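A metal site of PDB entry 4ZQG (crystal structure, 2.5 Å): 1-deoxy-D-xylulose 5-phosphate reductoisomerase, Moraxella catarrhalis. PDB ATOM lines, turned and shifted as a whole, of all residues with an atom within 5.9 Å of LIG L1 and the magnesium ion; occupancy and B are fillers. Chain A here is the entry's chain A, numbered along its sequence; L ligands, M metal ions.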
ATOM      1  N   LYS A 129      -8.533   2.720 -13.454  1.00  0.00           N
ATOM      2  CA  LYS A 129      -9.548   1.678 -13.112  1.00  0.00           C
ATOM      3  C   LYS A 129      -8.922   0.494 -12.362  1.00  0.00           C
ATOM      4  O   LYS A 129      -9.582  -0.135 -11.531  1.00  0.00           O
ATOM      5  CB  LYS A 129     -10.273   1.158 -14.368  1.00  0.00           C
ATOM      6  CG  LYS A 129      -9.321   0.462 -15.353  1.00  0.00           C
ATOM      7  CD  LYS A 129     -10.009   0.124 -16.652  1.00  0.00           C
ATOM      8  CE  LYS A 129     -10.539   1.352 -17.338  1.00  0.00           C
ATOM      9  NZ  LYS A 129     -10.779   1.064 -18.779  1.00  0.00           N
ATOM     10  N   ILE A 153     -14.181   9.063 -14.675  1.00  0.00           N
ATOM     11  CA  ILE A 153     -13.693   9.687 -15.880  1.00  0.00           C
ATOM     12  C   ILE A 153     -13.778   8.686 -16.978  1.00  0.00           C
ATOM     13  O   ILE A 153     -13.902   9.039 -18.143  1.00  0.00           O
ATOM     14  CB  ILE A 153     -12.191  10.067 -15.710  1.00  0.00           C
ATOM     15  CG1 ILE A 153     -12.057  11.473 -15.153  1.00  0.00           C
ATOM     16  CG2 ILE A 153     -11.346   9.902 -17.022  1.00  0.00           C
ATOM     17  CD1 ILE A 153     -10.582  11.839 -14.865  1.00  0.00           C
ATOM     18  N   ASP A 154     -13.617   7.409 -16.636  1.00  0.00           N
ATOM     19  CA  ASP A 154     -13.782   6.365 -17.602  1.00  0.00           C
ATOM     20  C   ASP A 154     -15.139   6.567 -18.353  1.00  0.00           C
ATOM     21  O   ASP A 154     -16.174   6.855 -17.729  1.00  0.00           O
ATOM     22  CB  ASP A 154     -13.691   4.989 -16.925  1.00  0.00           C
ATOM     23  CG  ASP A 154     -13.294   3.909 -17.915  1.00  0.00           C
ATOM     24  OD1 ASP A 154     -13.373   4.230 -19.100  1.00  0.00           O
ATOM     25  OD2 ASP A 154     -12.884   2.798 -17.528  1.00  0.00           O
ATOM     26  N   SER A 155     -15.117   6.456 -19.665  1.00  0.00           N
ATOM     27  CA  SER A 155     -16.256   6.812 -20.522  1.00  0.00           C
ATOM     28  C   SER A 155     -17.564   6.127 -20.126  1.00  0.00           C
ATOM     29  O   SER A 155     -18.566   6.782 -19.787  1.00  0.00           O
ATOM     30  CB  SER A 155     -15.947   6.467 -21.983  1.00  0.00           C
ATOM     31  OG  SER A 155     -16.771   7.200 -22.867  1.00  0.00           O
ATOM     32  N   GLU A 156     -17.509   4.804 -20.096  1.00  0.00           N
ATOM     33  CA  GLU A 156     -18.656   3.992 -19.739  1.00  0.00           C
ATOM     34  C   GLU A 156     -19.182   4.366 -18.369  1.00  0.00           C
ATOM     35  O   GLU A 156     -20.377   4.555 -18.198  1.00  0.00           O
ATOM     36  CB  GLU A 156     -18.326   2.523 -19.806  1.00  0.00           C
ATOM     37  CG  GLU A 156     -17.820   2.068 -21.178  1.00  0.00           C
ATOM     38  CD  GLU A 156     -16.355   2.377 -21.414  1.00  0.00           C
ATOM     39  OE1 GLU A 156     -15.820   2.040 -22.494  1.00  0.00           O
ATOM     40  OE2 GLU A 156     -15.761   2.954 -20.488  1.00  0.00           O
ATOM     41  N   HIS A 157     -18.303   4.527 -17.395  1.00  0.00           N
ATOM     42  CA  HIS A 157     -18.751   4.819 -16.048  1.00  0.00           C
ATOM     43  C   HIS A 157     -19.242   6.239 -15.943  1.00  0.00           C
ATOM     44  O   HIS A 157     -20.152   6.524 -15.149  1.00  0.00           O
ATOM     45  CB  HIS A 157     -17.626   4.567 -15.071  1.00  0.00           C
ATOM     46  CG  HIS A 157     -17.122   3.173 -15.153  1.00  0.00           C
ATOM     47  ND1 HIS A 157     -16.324   2.744 -16.191  1.00  0.00           N
ATOM     48  CD2 HIS A 157     -17.423   2.075 -14.434  1.00  0.00           C
ATOM     49  CE1 HIS A 157     -16.102   1.458 -16.064  1.00  0.00           C
ATOM     50  NE2 HIS A 157     -16.758   1.016 -15.002  1.00  0.00           N
ATOM     51  N   THR A 188     -21.229  -0.664 -22.873  1.00  0.00           N
ATOM     52  CA  THR A 188     -20.942  -0.780 -24.309  1.00  0.00           C
ATOM     53  C   THR A 188     -19.438  -1.132 -24.516  1.00  0.00           C
ATOM     54  O   THR A 188     -18.604  -0.712 -23.765  1.00  0.00           O
ATOM     55  CB  THR A 188     -21.307   0.537 -25.036  1.00  0.00           C
ATOM     56  OG1 THR A 188     -21.035   1.645 -24.142  1.00  0.00           O
ATOM     57  CG2 THR A 188     -22.772   0.552 -25.322  1.00  0.00           C
ATOM     58  N   ALA A 189     -19.135  -1.905 -25.545  1.00  0.00           N
ATOM     59  CA  ALA A 189     -17.792  -2.310 -25.859  1.00  0.00           C
ATOM     60  C   ALA A 189     -17.590  -2.217 -27.354  1.00  0.00           C
ATOM     61  O   ALA A 189     -18.434  -2.721 -28.136  1.00  0.00           O
ATOM     62  CB  ALA A 189     -17.618  -3.754 -25.447  1.00  0.00           C
ATOM     63  N   SER A 190     -16.478  -1.589 -27.776  1.00  0.00           N
ATOM     64  CA  SER A 190     -16.234  -1.431 -29.215  1.00  0.00           C
ATOM     65  C   SER A 190     -16.018  -2.763 -29.892  1.00  0.00           C
ATOM     66  O   SER A 190     -16.179  -2.885 -31.103  1.00  0.00           O
ATOM     67  CB  SER A 190     -15.025  -0.600 -29.510  1.00  0.00           C
ATOM     68  OG  SER A 190     -13.866  -1.385 -29.319  1.00  0.00           O
ATOM     69  N   GLY A 191     -15.603  -3.761 -29.126  1.00  0.00           N
ATOM     70  CA  GLY A 191     -15.213  -5.019 -29.702  1.00  0.00           C
ATOM     71  C   GLY A 191     -13.766  -5.009 -30.142  1.00  0.00           C
ATOM     72  O   GLY A 191     -13.262  -6.045 -30.551  1.00  0.00           O
ATOM     73  N   GLY A 192     -13.127  -3.832 -30.088  1.00  0.00           N
ATOM     74  CA  GLY A 192     -11.718  -3.624 -30.468  1.00  0.00           C
ATOM     75  C   GLY A 192     -11.340  -3.922 -31.902  1.00  0.00           C
ATOM     76  O   GLY A 192     -12.191  -4.218 -32.735  1.00  0.00           O
ATOM     77  N   HIS A 213      -6.420   1.477 -32.418  1.00  0.00           N
ATOM     78  CA  HIS A 213      -7.834   1.271 -32.213  1.00  0.00           C
ATOM     79  C   HIS A 213      -8.583   2.136 -33.216  1.00  0.00           C
ATOM     80  O   HIS A 213      -8.250   3.299 -33.353  1.00  0.00           O
ATOM     81  CB  HIS A 213      -8.204   1.675 -30.783  1.00  0.00           C
ATOM     82  CG  HIS A 213      -9.595   1.285 -30.365  1.00  0.00           C
ATOM     83  ND1 HIS A 213     -10.725   1.857 -30.918  1.00  0.00           N
ATOM     84  CD2 HIS A 213     -10.048   0.399 -29.446  1.00  0.00           C
ATOM     85  CE1 HIS A 213     -11.805   1.332 -30.368  1.00  0.00           C
ATOM     86  NE2 HIS A 213     -11.416   0.442 -29.475  1.00  0.00           N
ATOM     87  N   TRP A 216     -10.481   5.238 -30.896  1.00  0.00           N
ATOM     88  CA  TRP A 216      -9.904   5.879 -29.716  1.00  0.00           C
ATOM     89  C   TRP A 216      -8.385   5.957 -29.859  1.00  0.00           C
ATOM     90  O   TRP A 216      -7.789   5.056 -30.437  1.00  0.00           O
ATOM     91  CB  TRP A 216     -10.176   5.017 -28.486  1.00  0.00           C
ATOM     92  CG  TRP A 216     -11.521   4.993 -27.967  1.00  0.00           C
ATOM     93  CD1 TRP A 216     -12.417   3.966 -28.070  1.00  0.00           C
ATOM     94  CD2 TRP A 216     -12.144   5.998 -27.182  1.00  0.00           C
ATOM     95  NE1 TRP A 216     -13.570   4.285 -27.391  1.00  0.00           N
ATOM     96  CE2 TRP A 216     -13.429   5.525 -26.844  1.00  0.00           C
ATOM     97  CE3 TRP A 216     -11.750   7.267 -26.725  1.00  0.00           C
ATOM     98  CZ2 TRP A 216     -14.321   6.261 -26.093  1.00  0.00           C
ATOM     99  CZ3 TRP A 216     -12.641   8.000 -25.988  1.00  0.00           C
ATOM    100  CH2 TRP A 216     -13.915   7.499 -25.658  1.00  0.00           C
ATOM    101  N   MET A 218      -5.301   6.130 -27.143  1.00  0.00           N
ATOM    102  CA  MET A 218      -5.130   5.921 -25.713  1.00  0.00           C
ATOM    103  C   MET A 218      -3.736   5.445 -25.419  1.00  0.00           C
ATOM    104  O   MET A 218      -2.916   5.267 -26.328  1.00  0.00           O
ATOM    105  CB  MET A 218      -6.136   4.887 -25.227  1.00  0.00           C
ATOM    106  CG  MET A 218      -7.560   5.151 -25.675  1.00  0.00           C
ATOM    107  SD  MET A 218      -8.621   3.748 -25.289  1.00  0.00           S
ATOM    108  CE  MET A 218      -8.238   2.627 -26.641  1.00  0.00           C
ATOM    109  N   ILE A 222      -4.446  -0.023 -21.903  1.00  0.00           N
ATOM    110  CA  ILE A 222      -5.852   0.057 -22.196  1.00  0.00           C
ATOM    111  C   ILE A 222      -6.053  -0.255 -23.675  1.00  0.00           C
ATOM    112  O   ILE A 222      -6.970  -0.935 -24.044  1.00  0.00           O
ATOM    113  CB  ILE A 222      -6.482   1.412 -21.751  1.00  0.00           C
ATOM    114  CG1 ILE A 222      -7.982   1.249 -21.565  1.00  0.00           C
ATOM    115  CG2 ILE A 222      -6.254   2.522 -22.736  1.00  0.00           C
ATOM    116  CD1 ILE A 222      -8.690   2.458 -20.984  1.00  0.00           C
ATOM    117  N   SER A 226      -8.412  -3.450 -24.816  1.00  0.00           N
ATOM    118  CA  SER A 226      -9.575  -3.287 -25.663  1.00  0.00           C
ATOM    119  C   SER A 226      -9.577  -4.354 -26.765  1.00  0.00           C
ATOM    120  O   SER A 226     -10.583  -4.983 -27.018  1.00  0.00           O
ATOM    121  CB  SER A 226      -9.617  -1.873 -26.217  1.00  0.00           C
ATOM    122  OG  SER A 226     -10.607  -1.807 -27.198  1.00  0.00           O
ATOM    123  N   ALA A 227      -8.427  -4.579 -27.380  1.00  0.00           N
ATOM    124  CA  ALA A 227      -8.275  -5.672 -28.357  1.00  0.00           C
ATOM    125  C   ALA A 227      -8.741  -7.059 -27.848  1.00  0.00           C
ATOM    126  O   ALA A 227      -9.324  -7.805 -28.610  1.00  0.00           O
ATOM    127  CB  ALA A 227      -6.820  -5.738 -28.830  1.00  0.00           C
ATOM    128  N   MET A 229     -10.615  -7.522 -25.028  1.00  0.00           N
ATOM    129  CA  MET A 229     -11.840  -7.281 -24.309  1.00  0.00           C
ATOM    130  C   MET A 229     -11.708  -7.433 -22.800  1.00  0.00           C
ATOM    131  O   MET A 229     -12.682  -7.311 -22.062  1.00  0.00           O
ATOM    132  CB  MET A 229     -12.986  -8.143 -24.821  1.00  0.00           C
ATOM    133  CG  MET A 229     -14.349  -7.593 -24.397  1.00  0.00           C
ATOM    134  SD  MET A 229     -15.724  -7.711 -25.566  1.00  0.00           S
ATOM    135  CE  MET A 229     -14.896  -7.063 -27.010  1.00  0.00           C
ATOM    136  N   ASN A 231     -10.520  -5.074 -21.202  1.00  0.00           N
ATOM    137  CA  ASN A 231     -10.875  -3.720 -20.751  1.00  0.00           C
ATOM    138  C   ASN A 231     -12.328  -3.673 -20.229  1.00  0.00           C
ATOM    139  O   ASN A 231     -12.618  -3.030 -19.204  1.00  0.00           O
ATOM    140  CB  ASN A 231     -10.673  -2.700 -21.860  1.00  0.00           C
ATOM    141  CG  ASN A 231     -10.982  -1.274 -21.396  1.00  0.00           C
ATOM    142  OD1 ASN A 231     -10.444  -0.777 -20.400  1.00  0.00           O
ATOM    143  ND2 ASN A 231     -11.905  -0.628 -22.094  1.00  0.00           N
ATOM    144  N   LYS A 232     -13.226  -4.382 -20.904  1.00  0.00           N
ATOM    145  CA  LYS A 232     -14.598  -4.460 -20.453  1.00  0.00           C
ATOM    146  C   LYS A 232     -14.705  -5.265 -19.176  1.00  0.00           C
ATOM    147  O   LYS A 232     -15.452  -4.903 -18.273  1.00  0.00           O
ATOM    148  CB  LYS A 232     -15.491  -5.036 -21.531  1.00  0.00           C
ATOM    149  CG  LYS A 232     -16.825  -4.334 -21.639  1.00  0.00           C
ATOM    150  CD  LYS A 232     -16.735  -2.823 -21.567  1.00  0.00           C
ATOM    151  CE  LYS A 232     -15.811  -2.270 -22.644  1.00  0.00           C
ATOM    152  NZ  LYS A 232     -15.873  -0.786 -22.691  1.00  0.00           N
ATOM    153  N   GLU A 235     -13.680  -3.043 -16.486  1.00  0.00           N
ATOM    154  CA  GLU A 235     -14.715  -2.052 -16.367  1.00  0.00           C
ATOM    155  C   GLU A 235     -15.933  -2.629 -15.646  1.00  0.00           C
ATOM    156  O   GLU A 235     -16.570  -1.936 -14.836  1.00  0.00           O
ATOM    157  CB  GLU A 235     -15.054  -1.499 -17.744  1.00  0.00           C
ATOM    158  CG  GLU A 235     -14.017  -0.471 -18.148  1.00  0.00           C
ATOM    159  CD  GLU A 235     -14.215   0.059 -19.524  1.00  0.00           C
ATOM    160  OE1 GLU A 235     -15.180  -0.350 -20.215  1.00  0.00           O
ATOM    161  OE2 GLU A 235     -13.393   0.860 -19.900  1.00  0.00           O
ATOM    162  N   SER A 258     -18.709   3.082 -31.221  1.00  0.00           N
ATOM    163  CA  SER A 258     -18.249   3.865 -30.055  1.00  0.00           C
ATOM    164  C   SER A 258     -18.979   5.205 -29.833  1.00  0.00           C
ATOM    165  O   SER A 258     -18.418   6.163 -29.269  1.00  0.00           O
ATOM    166  CB  SER A 258     -16.714   4.009 -30.061  1.00  0.00           C
ATOM    167  OG  SER A 258     -16.104   2.788 -29.681  1.00  0.00           O
ATOM    168  N   MET A 280     -12.201  11.535 -24.820  1.00  0.00           N
ATOM    169  CA  MET A 280     -12.243  11.594 -23.365  1.00  0.00           C
ATOM    170  C   MET A 280     -12.384  12.986 -22.774  1.00  0.00           C
ATOM    171  O   MET A 280     -12.554  13.111 -21.585  1.00  0.00           O
ATOM    172  CB  MET A 280     -10.991  10.952 -22.771  1.00  0.00           C
ATOM    173  CG  MET A 280     -10.900   9.449 -22.981  1.00  0.00           C
ATOM    174  SD  MET A 280     -12.280   8.505 -22.312  1.00  0.00           S
ATOM    175  CE  MET A 280     -12.194   8.857 -20.562  1.00  0.00           C
HETATM  176  O1  LIG L   1     -12.136   2.421 -22.146  1.00  0.00           O
HETATM  177  N1  LIG L   1     -12.366   3.348 -23.153  1.00  0.00           N
HETATM  178  C1  LIG L   1     -12.965   4.440 -22.920  1.00  0.00           C
HETATM  179  O2  LIG L   1     -13.381   4.712 -21.807  1.00  0.00           O
HETATM  180  C2  LIG L   1     -11.923   2.924 -24.476  1.00  0.00           C
HETATM  181  C3  LIG L   1     -12.821   1.688 -24.644  1.00  0.00           C
HETATM  182  C4  LIG L   1     -12.445   0.886 -25.855  1.00  0.00           C
HETATM  183  P1  LIG L   1     -13.496  -0.553 -25.788  1.00  0.00           P
HETATM  184  O3  LIG L   1     -14.997  -0.033 -25.964  1.00  0.00           O
HETATM  185  O4  LIG L   1     -13.479  -1.099 -24.433  1.00  0.00           O
HETATM  186  O5  LIG L   1     -13.147  -1.717 -26.868  1.00  0.00           O
HETATM  187  P1  LG2 L   2      -0.687   6.303 -20.293  1.00  0.00           P
HETATM  188  O1  LG2 L   2       0.096   5.037 -20.409  1.00  0.00           O
HETATM  189  O2  LG2 L   2      -0.925   7.183 -21.501  1.00  0.00           O
HETATM  190  O3  LG2 L   2      -0.163   7.224 -19.073  1.00  0.00           O
HETATM  191  C1  LG2 L   2       0.025   6.755 -17.755  1.00  0.00           C
HETATM  192  C2  LG2 L   2       0.506   7.895 -16.829  1.00  0.00           C
HETATM  193  O4  LG2 L   2       0.859   7.287 -15.569  1.00  0.00           O
HETATM  194  C3  LG2 L   2       1.731   8.645 -17.351  1.00  0.00           C
HETATM  195  O5  LG2 L   2       1.687  10.038 -17.027  1.00  0.00           O
HETATM  196  C4  LG2 L   2       2.888   7.972 -16.613  1.00  0.00           C
HETATM  197  O6  LG2 L   2       3.939   8.869 -16.265  1.00  0.00           O
HETATM  198  C5  LG2 L   2       2.267   7.416 -15.341  1.00  0.00           C
HETATM  199  N1  LG2 L   2       2.891   6.117 -14.949  1.00  0.00           N
HETATM  200  C6  LG2 L   2       3.076   5.055 -15.765  1.00  0.00           C
HETATM  201  N2  LG2 L   2       3.677   4.036 -15.107  1.00  0.00           N
HETATM  202  C7  LG2 L   2       3.899   4.429 -13.851  1.00  0.00           C
HETATM  203  C8  LG2 L   2       4.521   3.789 -12.673  1.00  0.00           C
HETATM  204  N3  LG2 L   2       5.008   2.510 -12.747  1.00  0.00           N
HETATM  205  N4  LG2 L   2       4.560   4.549 -11.561  1.00  0.00           N
HETATM  206  C9  LG2 L   2       4.092   5.830 -11.516  1.00  0.00           C
HETATM  207  N5  LG2 L   2       3.520   6.481 -12.551  1.00  0.00           N
HETATM  208  C10 LG2 L   2       3.392   5.813 -13.738  1.00  0.00           C
HETATM  209  O7  LG2 L   2      -2.109   5.873 -19.663  1.00  0.00           O
HETATM  210  P2  LG2 L   2      -3.600   6.296 -20.085  1.00  0.00           P
HETATM  211  O8  LG2 L   2      -3.882   5.533 -21.368  1.00  0.00           O
HETATM  212  O9  LG2 L   2      -3.723   7.789 -19.918  1.00  0.00           O
HETATM  213  O10 LG2 L   2      -4.361   5.573 -18.869  1.00  0.00           O
HETATM  214  C11 LG2 L   2      -4.468   6.174 -17.583  1.00  0.00           C
HETATM  215  C12 LG2 L   2      -5.537   5.453 -16.752  1.00  0.00           C
HETATM  216  O11 LG2 L   2      -6.857   5.871 -17.126  1.00  0.00           O
HETATM  217  C13 LG2 L   2      -5.470   3.955 -16.963  1.00  0.00           C
HETATM  218  O12 LG2 L   2      -5.792   3.335 -15.727  1.00  0.00           O
HETATM  219  C14 LG2 L   2      -6.493   3.679 -18.036  1.00  0.00           C
HETATM  220  O13 LG2 L   2      -6.958   2.322 -17.985  1.00  0.00           O
HETATM  221  C15 LG2 L   2      -7.544   4.745 -17.717  1.00  0.00           C
HETATM  222  N6  LG2 L   2      -8.303   5.167 -18.911  1.00  0.00           N
HETATM  223  C16 LG2 L   2      -7.678   5.755 -19.966  1.00  0.00           C
HETATM  224  C17 LG2 L   2      -8.399   6.125 -21.117  1.00  0.00           C
HETATM  225  C18 LG2 L   2      -7.754   6.794 -22.300  1.00  0.00           C
HETATM  226  O14 LG2 L   2      -8.444   7.354 -23.133  1.00  0.00           O
HETATM  227  N7  LG2 L   2      -6.424   6.805 -22.430  1.00  0.00           N
HETATM  228  C19 LG2 L   2      -9.766   5.887 -21.158  1.00  0.00           C
HETATM  229  C20 LG2 L   2     -10.359   5.308 -20.061  1.00  0.00           C
HETATM  230  C21 LG2 L   2      -9.624   4.952 -18.942  1.00  0.00           C
HETATM  231 MG    MG M   1     -13.622   2.858 -20.679  1.00  0.00          MG
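OG of Ser 226 is in hydrogen-bond range of O5 of LIG L1 (2.6 Å).
An oxygen (O3) of LIG L1 lies within hydrogen-bond range of the backbone NH (N) of Ser 190, 2.8 Å away.
The side-chain hydroxyl (OG) of Ser 190 sits at hydrogen-bond distance from an oxygen (O5) of LIG L1 (2.6 Å).
O4 of LIG L1 sits at hydrogen-bond distance from ND2 of Asn 231, 2.9 Å away.
O4 of LIG L1 is in salt-bridge range of NZ of Lys 232 (3.0 Å).
The backbone NH (N) of Ser 155 lies close to an oxygen (O2) of LIG L1 (3.3 Å).
The side-chain carboxylate of Asp 154 lies within salt-bridge range of the side-chain amino group of Lys 129 (3.0 Å).
NZ of Lys 232 lies within salt-bridge range of OE1 of Glu 235 (2.6 Å).
The backbone carbonyl oxygen of Glu 235 sits at hydrogen-bond distance from a ring nitrogen (NE2) of His 157.
The side-chain hydroxyl (OG) of Ser 190 lies within hydrogen-bond range of a ring nitrogen (NE2) of His 213.
N of Gly 192 sits at hydrogen-bond distance from OG of Ser 190, 2.7 Å away.
The side-chain amide oxygen of Asn 231 is in hydrogen-bond range of the side-chain amino group of Lys 129, at 2.5 Å.
O of Thr 188 is in hydrogen-bond range of NZ of Lys 232, at 2.9 Å.
N of Trp 216 is in hydrogen-bond range of ND1 of His 213.
Residues that only touch LIG L1: Met 218, Ala 189, Trp 216, Ile 222, His 213, Gly 192, Lys 129, Gly 191 and Met 280.
The nearest printed residue that does not touch LIG L1 is Thr 188 (4.3 Å).
Merely in contact with the magnesium ion: Lys 129 (3.9 Å).
Within 4 Å of the magnesium ion: Lys 129, Asp 154, Glu 156 and Glu 235.
The magnesium ion is bound by the side-chain carboxylate of Asp 154 (2.1 Å), an oxygen (O1) of LIG L1 (2.1 Å), the side-chain carboxylate of Glu 156 (2.1 Å), the side-chain carboxylate of Glu 235 (2.2 Å) and an oxygen (O2) of LIG L1 (2.2 Å).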
